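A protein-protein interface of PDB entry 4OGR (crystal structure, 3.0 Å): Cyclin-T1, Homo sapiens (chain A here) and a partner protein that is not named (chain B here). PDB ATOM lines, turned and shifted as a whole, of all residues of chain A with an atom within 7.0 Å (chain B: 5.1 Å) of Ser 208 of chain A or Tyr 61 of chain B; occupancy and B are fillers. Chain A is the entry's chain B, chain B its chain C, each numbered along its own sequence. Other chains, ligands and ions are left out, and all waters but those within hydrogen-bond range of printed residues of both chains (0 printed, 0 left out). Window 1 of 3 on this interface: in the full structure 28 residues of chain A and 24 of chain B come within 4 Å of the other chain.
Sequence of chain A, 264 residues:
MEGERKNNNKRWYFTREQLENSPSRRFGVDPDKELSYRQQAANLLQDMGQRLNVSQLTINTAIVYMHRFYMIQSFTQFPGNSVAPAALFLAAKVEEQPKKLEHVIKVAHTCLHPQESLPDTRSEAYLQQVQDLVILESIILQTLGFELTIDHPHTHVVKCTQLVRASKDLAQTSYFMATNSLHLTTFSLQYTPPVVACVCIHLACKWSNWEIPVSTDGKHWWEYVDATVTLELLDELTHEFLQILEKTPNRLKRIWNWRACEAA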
ATOM      1  N   SER A 167      22.203  -6.105  13.893  1.00  0.00           N
ATOM      2  CA  SER A 167      21.046  -6.940  14.186  1.00  0.00           C
ATOM      3  C   SER A 167      19.991  -6.792  13.092  1.00  0.00           C
ATOM      4  O   SER A 167      20.075  -5.875  12.275  1.00  0.00           O
ATOM      5  CB  SER A 167      20.463  -6.563  15.541  1.00  0.00           C
ATOM      6  OG  SER A 167      20.333  -5.155  15.647  1.00  0.00           O
ATOM      7  N   LYS A 168      19.001  -7.682  13.077  1.00  0.00           N
ATOM      8  CA  LYS A 168      17.948  -7.624  12.065  1.00  0.00           C
ATOM      9  C   LYS A 168      17.218  -6.289  12.090  1.00  0.00           C
ATOM     10  O   LYS A 168      16.897  -5.729  11.041  1.00  0.00           O
ATOM     11  CB  LYS A 168      16.932  -8.755  12.258  1.00  0.00           C
ATOM     12  CG  LYS A 168      17.340 -10.078  11.631  1.00  0.00           C
ATOM     13  CD  LYS A 168      16.132 -10.920  11.215  1.00  0.00           C
ATOM     14  CE  LYS A 168      15.425 -10.354   9.984  1.00  0.00           C
ATOM     15  NZ  LYS A 168      14.164  -9.640  10.329  1.00  0.00           N
ATOM     16  N   ASP A 169      16.960  -5.774  13.287  1.00  0.00           N
ATOM     17  CA  ASP A 169      16.221  -4.526  13.406  1.00  0.00           C
ATOM     18  C   ASP A 169      17.039  -3.376  12.826  1.00  0.00           C
ATOM     19  O   ASP A 169      16.506  -2.528  12.109  1.00  0.00           O
ATOM     20  CB  ASP A 169      15.846  -4.245  14.869  1.00  0.00           C
ATOM     21  CG  ASP A 169      17.057  -4.031  15.762  1.00  0.00           C
ATOM     22  OD1 ASP A 169      17.628  -5.032  16.247  1.00  0.00           O
ATOM     23  OD2 ASP A 169      17.431  -2.858  15.985  1.00  0.00           O
ATOM     24  N   LEU A 170      18.339  -3.367  13.103  1.00  0.00           N
ATOM     25  CA  LEU A 170      19.197  -2.297  12.616  1.00  0.00           C
ATOM     26  C   LEU A 170      19.360  -2.398  11.107  1.00  0.00           C
ATOM     27  O   LEU A 170      19.400  -1.384  10.408  1.00  0.00           O
ATOM     28  CB  LEU A 170      20.559  -2.336  13.309  1.00  0.00           C
ATOM     29  CG  LEU A 170      21.572  -1.273  12.867  1.00  0.00           C
ATOM     30  CD1 LEU A 170      20.972   0.132  12.884  1.00  0.00           C
ATOM     31  CD2 LEU A 170      22.802  -1.327  13.756  1.00  0.00           C
ATOM     32  N   ALA A 171      19.444  -3.627  10.608  1.00  0.00           N
ATOM     33  CA  ALA A 171      19.501  -3.864   9.174  1.00  0.00           C
ATOM     34  C   ALA A 171      18.202  -3.395   8.525  1.00  0.00           C
ATOM     35  O   ALA A 171      18.218  -2.661   7.533  1.00  0.00           O
ATOM     36  CB  ALA A 171      19.739  -5.331   8.889  1.00  0.00           C
ATOM     37  N   GLN A 172      17.081  -3.822   9.102  1.00  0.00           N
ATOM     38  CA  GLN A 172      15.760  -3.410   8.637  1.00  0.00           C
ATOM     39  C   GLN A 172      15.607  -1.890   8.606  1.00  0.00           C
ATOM     40  O   GLN A 172      15.173  -1.320   7.604  1.00  0.00           O
ATOM     41  CB  GLN A 172      14.676  -4.013   9.530  1.00  0.00           C
ATOM     42  CG  GLN A 172      14.369  -5.476   9.248  1.00  0.00           C
ATOM     43  CD  GLN A 172      13.393  -6.100  10.242  1.00  0.00           C
ATOM     44  OE1 GLN A 172      12.831  -7.161   9.970  1.00  0.00           O
ATOM     45  NE2 GLN A 172      13.184  -5.450  11.394  1.00  0.00           N
ATOM     46  N   THR A 173      15.958  -1.242   9.712  1.00  0.00           N
ATOM     47  CA  THR A 173      15.771   0.199   9.843  1.00  0.00           C
ATOM     48  C   THR A 173      16.638   0.973   8.855  1.00  0.00           C
ATOM     49  O   THR A 173      16.163   1.910   8.217  1.00  0.00           O
ATOM     50  CB  THR A 173      16.080   0.673  11.276  1.00  0.00           C
ATOM     51  OG1 THR A 173      15.242  -0.027  12.205  1.00  0.00           O
ATOM     52  CG2 THR A 173      15.844   2.176  11.417  1.00  0.00           C
ATOM     53  N   SER A 174      17.900   0.580   8.723  1.00  0.00           N
ATOM     54  CA  SER A 174      18.811   1.249   7.797  1.00  0.00           C
ATOM     55  C   SER A 174      18.268   1.181   6.372  1.00  0.00           C
ATOM     56  O   SER A 174      18.218   2.184   5.658  1.00  0.00           O
ATOM     57  CB  SER A 174      20.201   0.616   7.862  1.00  0.00           C
ATOM     58  OG  SER A 174      20.724   0.684   9.177  1.00  0.00           O
ATOM     59  N   ILE A 201      22.338   4.643   7.607  1.00  0.00           N
ATOM     60  CA  ILE A 201      22.860   3.844   8.711  1.00  0.00           C
ATOM     61  C   ILE A 201      23.140   4.728   9.923  1.00  0.00           C
ATOM     62  O   ILE A 201      22.811   4.370  11.055  1.00  0.00           O
ATOM     63  CB  ILE A 201      24.140   3.092   8.293  1.00  0.00           C
ATOM     64  CG1 ILE A 201      23.774   1.960   7.335  1.00  0.00           C
ATOM     65  CG2 ILE A 201      24.881   2.537   9.508  1.00  0.00           C
ATOM     66  CD1 ILE A 201      24.964   1.271   6.693  1.00  0.00           C
ATOM     67  N   LEU A 203      21.752   7.516  10.723  1.00  0.00           N
ATOM     68  CA  LEU A 203      20.479   7.941  11.290  1.00  0.00           C
ATOM     69  C   LEU A 203      19.821   6.811  12.075  1.00  0.00           C
ATOM     70  O   LEU A 203      19.291   7.031  13.164  1.00  0.00           O
ATOM     71  CB  LEU A 203      19.555   8.434  10.175  1.00  0.00           C
ATOM     72  CG  LEU A 203      18.145   8.917  10.519  1.00  0.00           C
ATOM     73  CD1 LEU A 203      18.100   9.719  11.808  1.00  0.00           C
ATOM     74  CD2 LEU A 203      17.632   9.771   9.375  1.00  0.00           C
ATOM     75  N   ALA A 204      19.866   5.601  11.531  1.00  0.00           N
ATOM     76  CA  ALA A 204      19.275   4.452  12.203  1.00  0.00           C
ATOM     77  C   ALA A 204      19.978   4.179  13.530  1.00  0.00           C
ATOM     78  O   ALA A 204      19.347   3.772  14.505  1.00  0.00           O
ATOM     79  CB  ALA A 204      19.338   3.225  11.310  1.00  0.00           C
ATOM     80  N   CYS A 205      21.283   4.428  13.569  1.00  0.00           N
ATOM     81  CA  CYS A 205      22.068   4.185  14.773  1.00  0.00           C
ATOM     82  C   CYS A 205      21.747   5.195  15.866  1.00  0.00           C
ATOM     83  O   CYS A 205      21.556   4.827  17.025  1.00  0.00           O
ATOM     84  CB  CYS A 205      23.562   4.226  14.453  1.00  0.00           C
ATOM     85  SG  CYS A 205      24.185   2.734  13.652  1.00  0.00           S
ATOM     86  N   LYS A 206      21.694   6.470  15.493  1.00  0.00           N
ATOM     87  CA  LYS A 206      21.417   7.537  16.445  1.00  0.00           C
ATOM     88  C   LYS A 206      20.025   7.378  17.049  1.00  0.00           C
ATOM     89  O   LYS A 206      19.797   7.717  18.212  1.00  0.00           O
ATOM     90  CB  LYS A 206      21.545   8.904  15.765  1.00  0.00           C
ATOM     91  CG  LYS A 206      22.943   9.223  15.256  1.00  0.00           C
ATOM     92  CD  LYS A 206      23.925   9.465  16.390  1.00  0.00           C
ATOM     93  CE  LYS A 206      25.330   9.704  15.855  1.00  0.00           C
ATOM     94  NZ  LYS A 206      26.346   9.787  16.942  1.00  0.00           N
ATOM     95  N   TRP A 207      19.096   6.862  16.252  1.00  0.00           N
ATOM     96  CA  TRP A 207      17.733   6.628  16.717  1.00  0.00           C
ATOM     97  C   TRP A 207      17.670   5.444  17.680  1.00  0.00           C
ATOM     98  O   TRP A 207      17.098   5.542  18.765  1.00  0.00           O
ATOM     99  CB  TRP A 207      16.804   6.385  15.525  1.00  0.00           C
ATOM    100  CG  TRP A 207      15.355   6.267  15.894  1.00  0.00           C
ATOM    101  CD1 TRP A 207      14.763   6.697  17.046  1.00  0.00           C
ATOM    102  CD2 TRP A 207      14.313   5.678  15.105  1.00  0.00           C
ATOM    103  NE1 TRP A 207      13.419   6.412  17.024  1.00  0.00           N
ATOM    104  CE2 TRP A 207      13.118   5.788  15.844  1.00  0.00           C
ATOM    105  CE3 TRP A 207      14.276   5.069  13.849  1.00  0.00           C
ATOM    106  CZ2 TRP A 207      11.899   5.310  15.366  1.00  0.00           C
ATOM    107  CZ3 TRP A 207      13.066   4.596  13.377  1.00  0.00           C
ATOM    108  CH2 TRP A 207      11.894   4.720  14.134  1.00  0.00           C
ATOM    109  N   SER A 208      18.285   4.334  17.276  1.00  0.00           N
ATOM    110  CA  SER A 208      18.192   3.069  18.006  1.00  0.00           C
ATOM    111  C   SER A 208      19.153   2.970  19.184  1.00  0.00           C
ATOM    112  O   SER A 208      19.041   2.054  19.997  1.00  0.00           O
ATOM    113  CB  SER A 208      18.458   1.903  17.057  1.00  0.00           C
ATOM    114  OG  SER A 208      19.771   1.983  16.532  1.00  0.00           O
ATOM    115  N   ASN A 209      20.105   3.897  19.251  1.00  0.00           N
ATOM    116  CA  ASN A 209      21.188   3.868  20.236  1.00  0.00           C
ATOM    117  C   ASN A 209      22.113   2.667  20.062  1.00  0.00           C
ATOM    118  O   ASN A 209      22.936   2.383  20.931  1.00  0.00           O
ATOM    119  CB  ASN A 209      20.636   3.887  21.665  1.00  0.00           C
ATOM    120  CG  ASN A 209      19.931   5.180  21.995  1.00  0.00           C
ATOM    121  OD1 ASN A 209      18.740   5.192  22.306  1.00  0.00           O
ATOM    122  ND2 ASN A 209      20.665   6.284  21.931  1.00  0.00           N
ATOM    123  N   TRP A 210      21.975   1.955  18.947  1.00  0.00           N
ATOM    124  CA  TRP A 210      23.003   1.006  18.544  1.00  0.00           C
ATOM    125  C   TRP A 210      24.245   1.818  18.210  1.00  0.00           C
ATOM    126  O   TRP A 210      24.138   2.889  17.612  1.00  0.00           O
ATOM    127  CB  TRP A 210      22.579   0.174  17.332  1.00  0.00           C
ATOM    128  CG  TRP A 210      21.619  -0.949  17.618  1.00  0.00           C
ATOM    129  CD1 TRP A 210      20.395  -1.138  17.045  1.00  0.00           C
ATOM    130  CD2 TRP A 210      21.804  -2.039  18.532  1.00  0.00           C
ATOM    131  NE1 TRP A 210      19.809  -2.275  17.542  1.00  0.00           N
ATOM    132  CE2 TRP A 210      20.652  -2.847  18.457  1.00  0.00           C
ATOM    133  CE3 TRP A 210      22.830  -2.411  19.405  1.00  0.00           C
ATOM    134  CZ2 TRP A 210      20.497  -4.001  19.221  1.00  0.00           C
ATOM    135  CZ3 TRP A 210      22.673  -3.560  20.163  1.00  0.00           C
ATOM    136  CH2 TRP A 210      21.515  -4.338  20.066  1.00  0.00           C
ATOM    137  N   GLU A 211      25.414   1.314  18.590  1.00  0.00           N
ATOM    138  CA  GLU A 211      26.673   1.967  18.257  1.00  0.00           C
ATOM    139  C   GLU A 211      27.600   1.011  17.531  1.00  0.00           C
ATOM    140  O   GLU A 211      27.840  -0.107  17.989  1.00  0.00           O
ATOM    141  CB  GLU A 211      27.360   2.494  19.514  1.00  0.00           C
ATOM    142  CG  GLU A 211      28.778   2.977  19.273  1.00  0.00           C
ATOM    143  CD  GLU A 211      29.311   3.819  20.413  1.00  0.00           C
ATOM    144  OE1 GLU A 211      28.753   4.910  20.657  1.00  0.00           O
ATOM    145  OE2 GLU A 211      30.283   3.389  21.068  1.00  0.00           O
ATOM    146  N   LYS B  42      24.475  -1.307  22.646  1.00  0.00           N
ATOM    147  CA  LYS B  42      23.640  -0.177  23.031  1.00  0.00           C
ATOM    148  C   LYS B  42      24.465   0.883  23.743  1.00  0.00           C
ATOM    149  O   LYS B  42      25.476   0.575  24.374  1.00  0.00           O
ATOM    150  CB  LYS B  42      22.490  -0.628  23.934  1.00  0.00           C
ATOM    151  CG  LYS B  42      21.450  -1.496  23.255  1.00  0.00           C
ATOM    152  CD  LYS B  42      20.731  -0.747  22.144  1.00  0.00           C
ATOM    153  CE  LYS B  42      19.568  -1.560  21.596  1.00  0.00           C
ATOM    154  NZ  LYS B  42      18.981  -0.953  20.370  1.00  0.00           N
ATOM    155  N   GLN B  55      15.205  11.148  18.558  1.00  0.00           N
ATOM    156  CA  GLN B  55      14.327  10.397  19.446  1.00  0.00           C
ATOM    157  C   GLN B  55      13.083  11.206  19.815  1.00  0.00           C
ATOM    158  O   GLN B  55      12.000  10.649  19.991  1.00  0.00           O
ATOM    159  CB  GLN B  55      15.080   9.985  20.713  1.00  0.00           C
ATOM    160  CG  GLN B  55      16.467   9.394  20.445  1.00  0.00           C
ATOM    161  CD  GLN B  55      16.728   8.070  21.148  1.00  0.00           C
ATOM    162  OE1 GLN B  55      15.839   7.480  21.763  1.00  0.00           O
ATOM    163  NE2 GLN B  55      17.963   7.594  21.048  1.00  0.00           N
ATOM    164  N   GLY B  59      10.342   9.285  18.030  1.00  0.00           N
ATOM    165  CA  GLY B  59       9.848   8.621  19.222  1.00  0.00           C
ATOM    166  C   GLY B  59      10.828   7.592  19.751  1.00  0.00           C
ATOM    167  O   GLY B  59      12.040   7.737  19.592  1.00  0.00           O
ATOM    168  N   ASN B  60      10.296   6.539  20.364  1.00  0.00           N
ATOM    169  CA  ASN B  60      11.120   5.500  20.967  1.00  0.00           C
ATOM    170  C   ASN B  60      11.324   4.356  19.984  1.00  0.00           C
ATOM    171  O   ASN B  60      10.362   3.738  19.530  1.00  0.00           O
ATOM    172  CB  ASN B  60      10.475   4.990  22.260  1.00  0.00           C
ATOM    173  CG  ASN B  60      11.290   3.900  22.931  1.00  0.00           C
ATOM    174  OD1 ASN B  60      12.488   3.762  22.688  1.00  0.00           O
ATOM    175  ND2 ASN B  60      10.641   3.123  23.788  1.00  0.00           N
ATOM    176  N   TYR B  61      12.583   4.087  19.649  1.00  0.00           N
ATOM    177  CA  TYR B  61      12.909   3.120  18.609  1.00  0.00           C
ATOM    178  C   TYR B  61      12.371   1.722  18.904  1.00  0.00           C
ATOM    179  O   TYR B  61      11.799   1.081  18.026  1.00  0.00           O
ATOM    180  CB  TYR B  61      14.421   3.047  18.408  1.00  0.00           C
ATOM    181  CG  TYR B  61      14.834   1.968  17.436  1.00  0.00           C
ATOM    182  CD1 TYR B  61      14.688   2.147  16.066  1.00  0.00           C
ATOM    183  CD2 TYR B  61      15.362   0.767  17.887  1.00  0.00           C
ATOM    184  CE1 TYR B  61      15.060   1.163  15.174  1.00  0.00           C
ATOM    185  CE2 TYR B  61      15.737  -0.225  17.003  1.00  0.00           C
ATOM    186  CZ  TYR B  61      15.584  -0.022  15.647  1.00  0.00           C
ATOM    187  OH  TYR B  61      15.957  -1.007  14.763  1.00  0.00           O
ATOM    188  N   ASP B  62      12.553   1.252  20.133  1.00  0.00           N
ATOM    189  CA  ASP B  62      12.202  -0.124  20.472  1.00  0.00           C
ATOM    190  C   ASP B  62      10.699  -0.352  20.365  1.00  0.00           C
ATOM    191  O   ASP B  62      10.249  -1.478  20.153  1.00  0.00           O
ATOM    192  CB  ASP B  62      12.695  -0.472  21.879  1.00  0.00           C
ATOM    193  CG  ASP B  62      14.202  -0.323  22.023  1.00  0.00           C
ATOM    194  OD1 ASP B  62      14.663   0.798  22.327  1.00  0.00           O
ATOM    195  OD2 ASP B  62      14.928  -1.323  21.829  1.00  0.00           O
ATOM    196  N   GLU B  63       9.926   0.720  20.506  1.00  0.00           N
ATOM    197  CA  GLU B  63       8.479   0.648  20.341  1.00  0.00           C
ATOM    198  C   GLU B  63       8.085   0.449  18.877  1.00  0.00           C
ATOM    199  O   GLU B  63       6.960   0.050  18.582  1.00  0.00           O
ATOM    200  CB  GLU B  63       7.817   1.915  20.884  1.00  0.00           C
ATOM    201  CG  GLU B  63       7.440   1.847  22.354  1.00  0.00           C
ATOM    202  CD  GLU B  63       7.406   3.214  23.015  1.00  0.00           C
ATOM    203  OE1 GLU B  63       7.113   4.207  22.317  1.00  0.00           O
ATOM    204  OE2 GLU B  63       7.667   3.291  24.236  1.00  0.00           O
ATOM    205  N   MET B  64       9.019   0.728  17.969  1.00  0.00           N
ATOM    206  CA  MET B  64       8.741   0.743  16.530  1.00  0.00           C
ATOM    207  C   MET B  64       9.443  -0.386  15.777  1.00  0.00           C
ATOM    208  O   MET B  64       8.971  -0.827  14.729  1.00  0.00           O
ATOM    209  CB  MET B  64       9.172   2.083  15.922  1.00  0.00           C
ATOM    210  CG  MET B  64       8.690   3.315  16.677  1.00  0.00           C
ATOM    211  SD  MET B  64       6.948   3.699  16.415  1.00  0.00           S
ATOM    212  CE  MET B  64       7.029   5.488  16.400  1.00  0.00           C
ATOM    213  N   LYS B  65      10.580  -0.829  16.307  1.00  0.00           N
ATOM    214  CA  LYS B  65      11.486  -1.723  15.589  1.00  0.00           C
ATOM    215  C   LYS B  65      10.807  -2.988  15.055  1.00  0.00           C
ATOM    216  O   LYS B  65      11.197  -3.510  14.009  1.00  0.00           O
ATOM    217  CB  LYS B  65      12.665  -2.096  16.497  1.00  0.00           C
ATOM    218  CG  LYS B  65      12.391  -3.214  17.494  1.00  0.00           C
ATOM    219  CD  LYS B  65      13.495  -3.296  18.545  1.00  0.00           C
ATOM    220  CE  LYS B  65      13.012  -3.928  19.848  1.00  0.00           C
ATOM    221  NZ  LYS B  65      12.851  -5.409  19.766  1.00  0.00           N
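O of Ser 208 of chain A is in hydrogen-bond range of NZ of Lys 42 of chain B. The side-chain amide oxygen (OD1) of Asn 209 of chain A is in hydrogen-bond range of the side-chain amide nitrogen (NE2) of Gln 55 of chain B, 2.8 Å away. The indole nitrogen (NE1) of Trp 210 of chain A sits close to the side-chain amino group (NZ) of Lys 42 of chain B (3.2 Å). The side-chain hydroxyl of Thr 173 of chain A sits at hydrogen-bond distance from the side-chain hydroxyl of Tyr 61 of chain B. O of Lys 206 of chain A lies within hydrogen-bond range of NE2 of Gln 55 of chain B, 3.4 Å away. O of Trp 207 of chain A lies within hydrogen-bond range of NE2 of Gln 55 of chain B (3.2 Å). OD2 of Asp 169 of chain A lies within hydrogen-bond range of OH of Tyr 61 of chain B, 2.7 Å away. The indole nitrogen (NE1) of Trp 207 of chain A is in hydrogen-bond range of the backbone carbonyl oxygen (O) of Gly 59 of chain B (3.2 Å).
OG of Ser 208 of chain A lies within hydrogen-bond range of O of Ala 204 of chain A (2.7 Å). OE1 of Gln 172 of chain A is in hydrogen-bond range of NZ of Lys 168 of chain A. The side-chain hydroxyl (OG) of Ser 167 of chain A sits at hydrogen-bond distance from the indole nitrogen (NE1) of Trp 210 of chain A. The side-chain carboxylate (OD1) of Asp 169 of chain A sits at hydrogen-bond distance from the side-chain hydroxyl (OG) of Ser 167 of chain A (2.8 Å). The backbone carbonyl oxygen (O) of Cys 205 of chain A is in hydrogen-bond range of the side-chain hydroxyl (OG) of Ser 208 of chain A. O of Cys 205 of chain A is in hydrogen-bond range of N of Trp 210 of chain A (3.5 Å).
Among the printed residues, merely in contact across the chains: Asn 209 of chain A with Lys 42 of chain B (3.4 Å), Ser 208 of chain A with Tyr 61 of chain B (3.4 Å), Trp 207 of chain A with Tyr 61 of chain B (3.6 Å), Leu 170 of chain A with Tyr 61 of chain B (3.7 Å), Gln 172 of chain A with Lys 65 of chain B (3.8 Å) and Trp 207 of chain A with Met 64 of chain B (3.9996 Å).
Ala 171 of chain A touches none of the printed residues of chain B. Of the printed residues of chain B, Ser 208 of chain A touches Lys 42 and Tyr 61. Of the printed residues of chain A, Gln 55 of chain B touches Lys 206, Trp 207 and Asn 209. Asn 60 of chain B touches none of the printed residues of chain A. Of the printed residues of chain A, Lys 65 of chain B touches Gln 172 (3.8 Å). The nearest residue of chain B that does not touch Ser 208 of chain A is Gln 55 of chain B (5.0 Å). The nearest residue of chain A that does not touch Tyr 61 of chain B is Trp 210 of chain A (4.6 Å).
Hydrophobic or aromatic side chains of chain A within 4 Å of the printed part of chain B: Trp 207 and Trp 210. Hydrophobic or aromatic side chains of chain B within 4 Å of the printed part of chain A: Tyr 61 and Met 64. Among the printed residues, 14 pairs touch across the chains.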
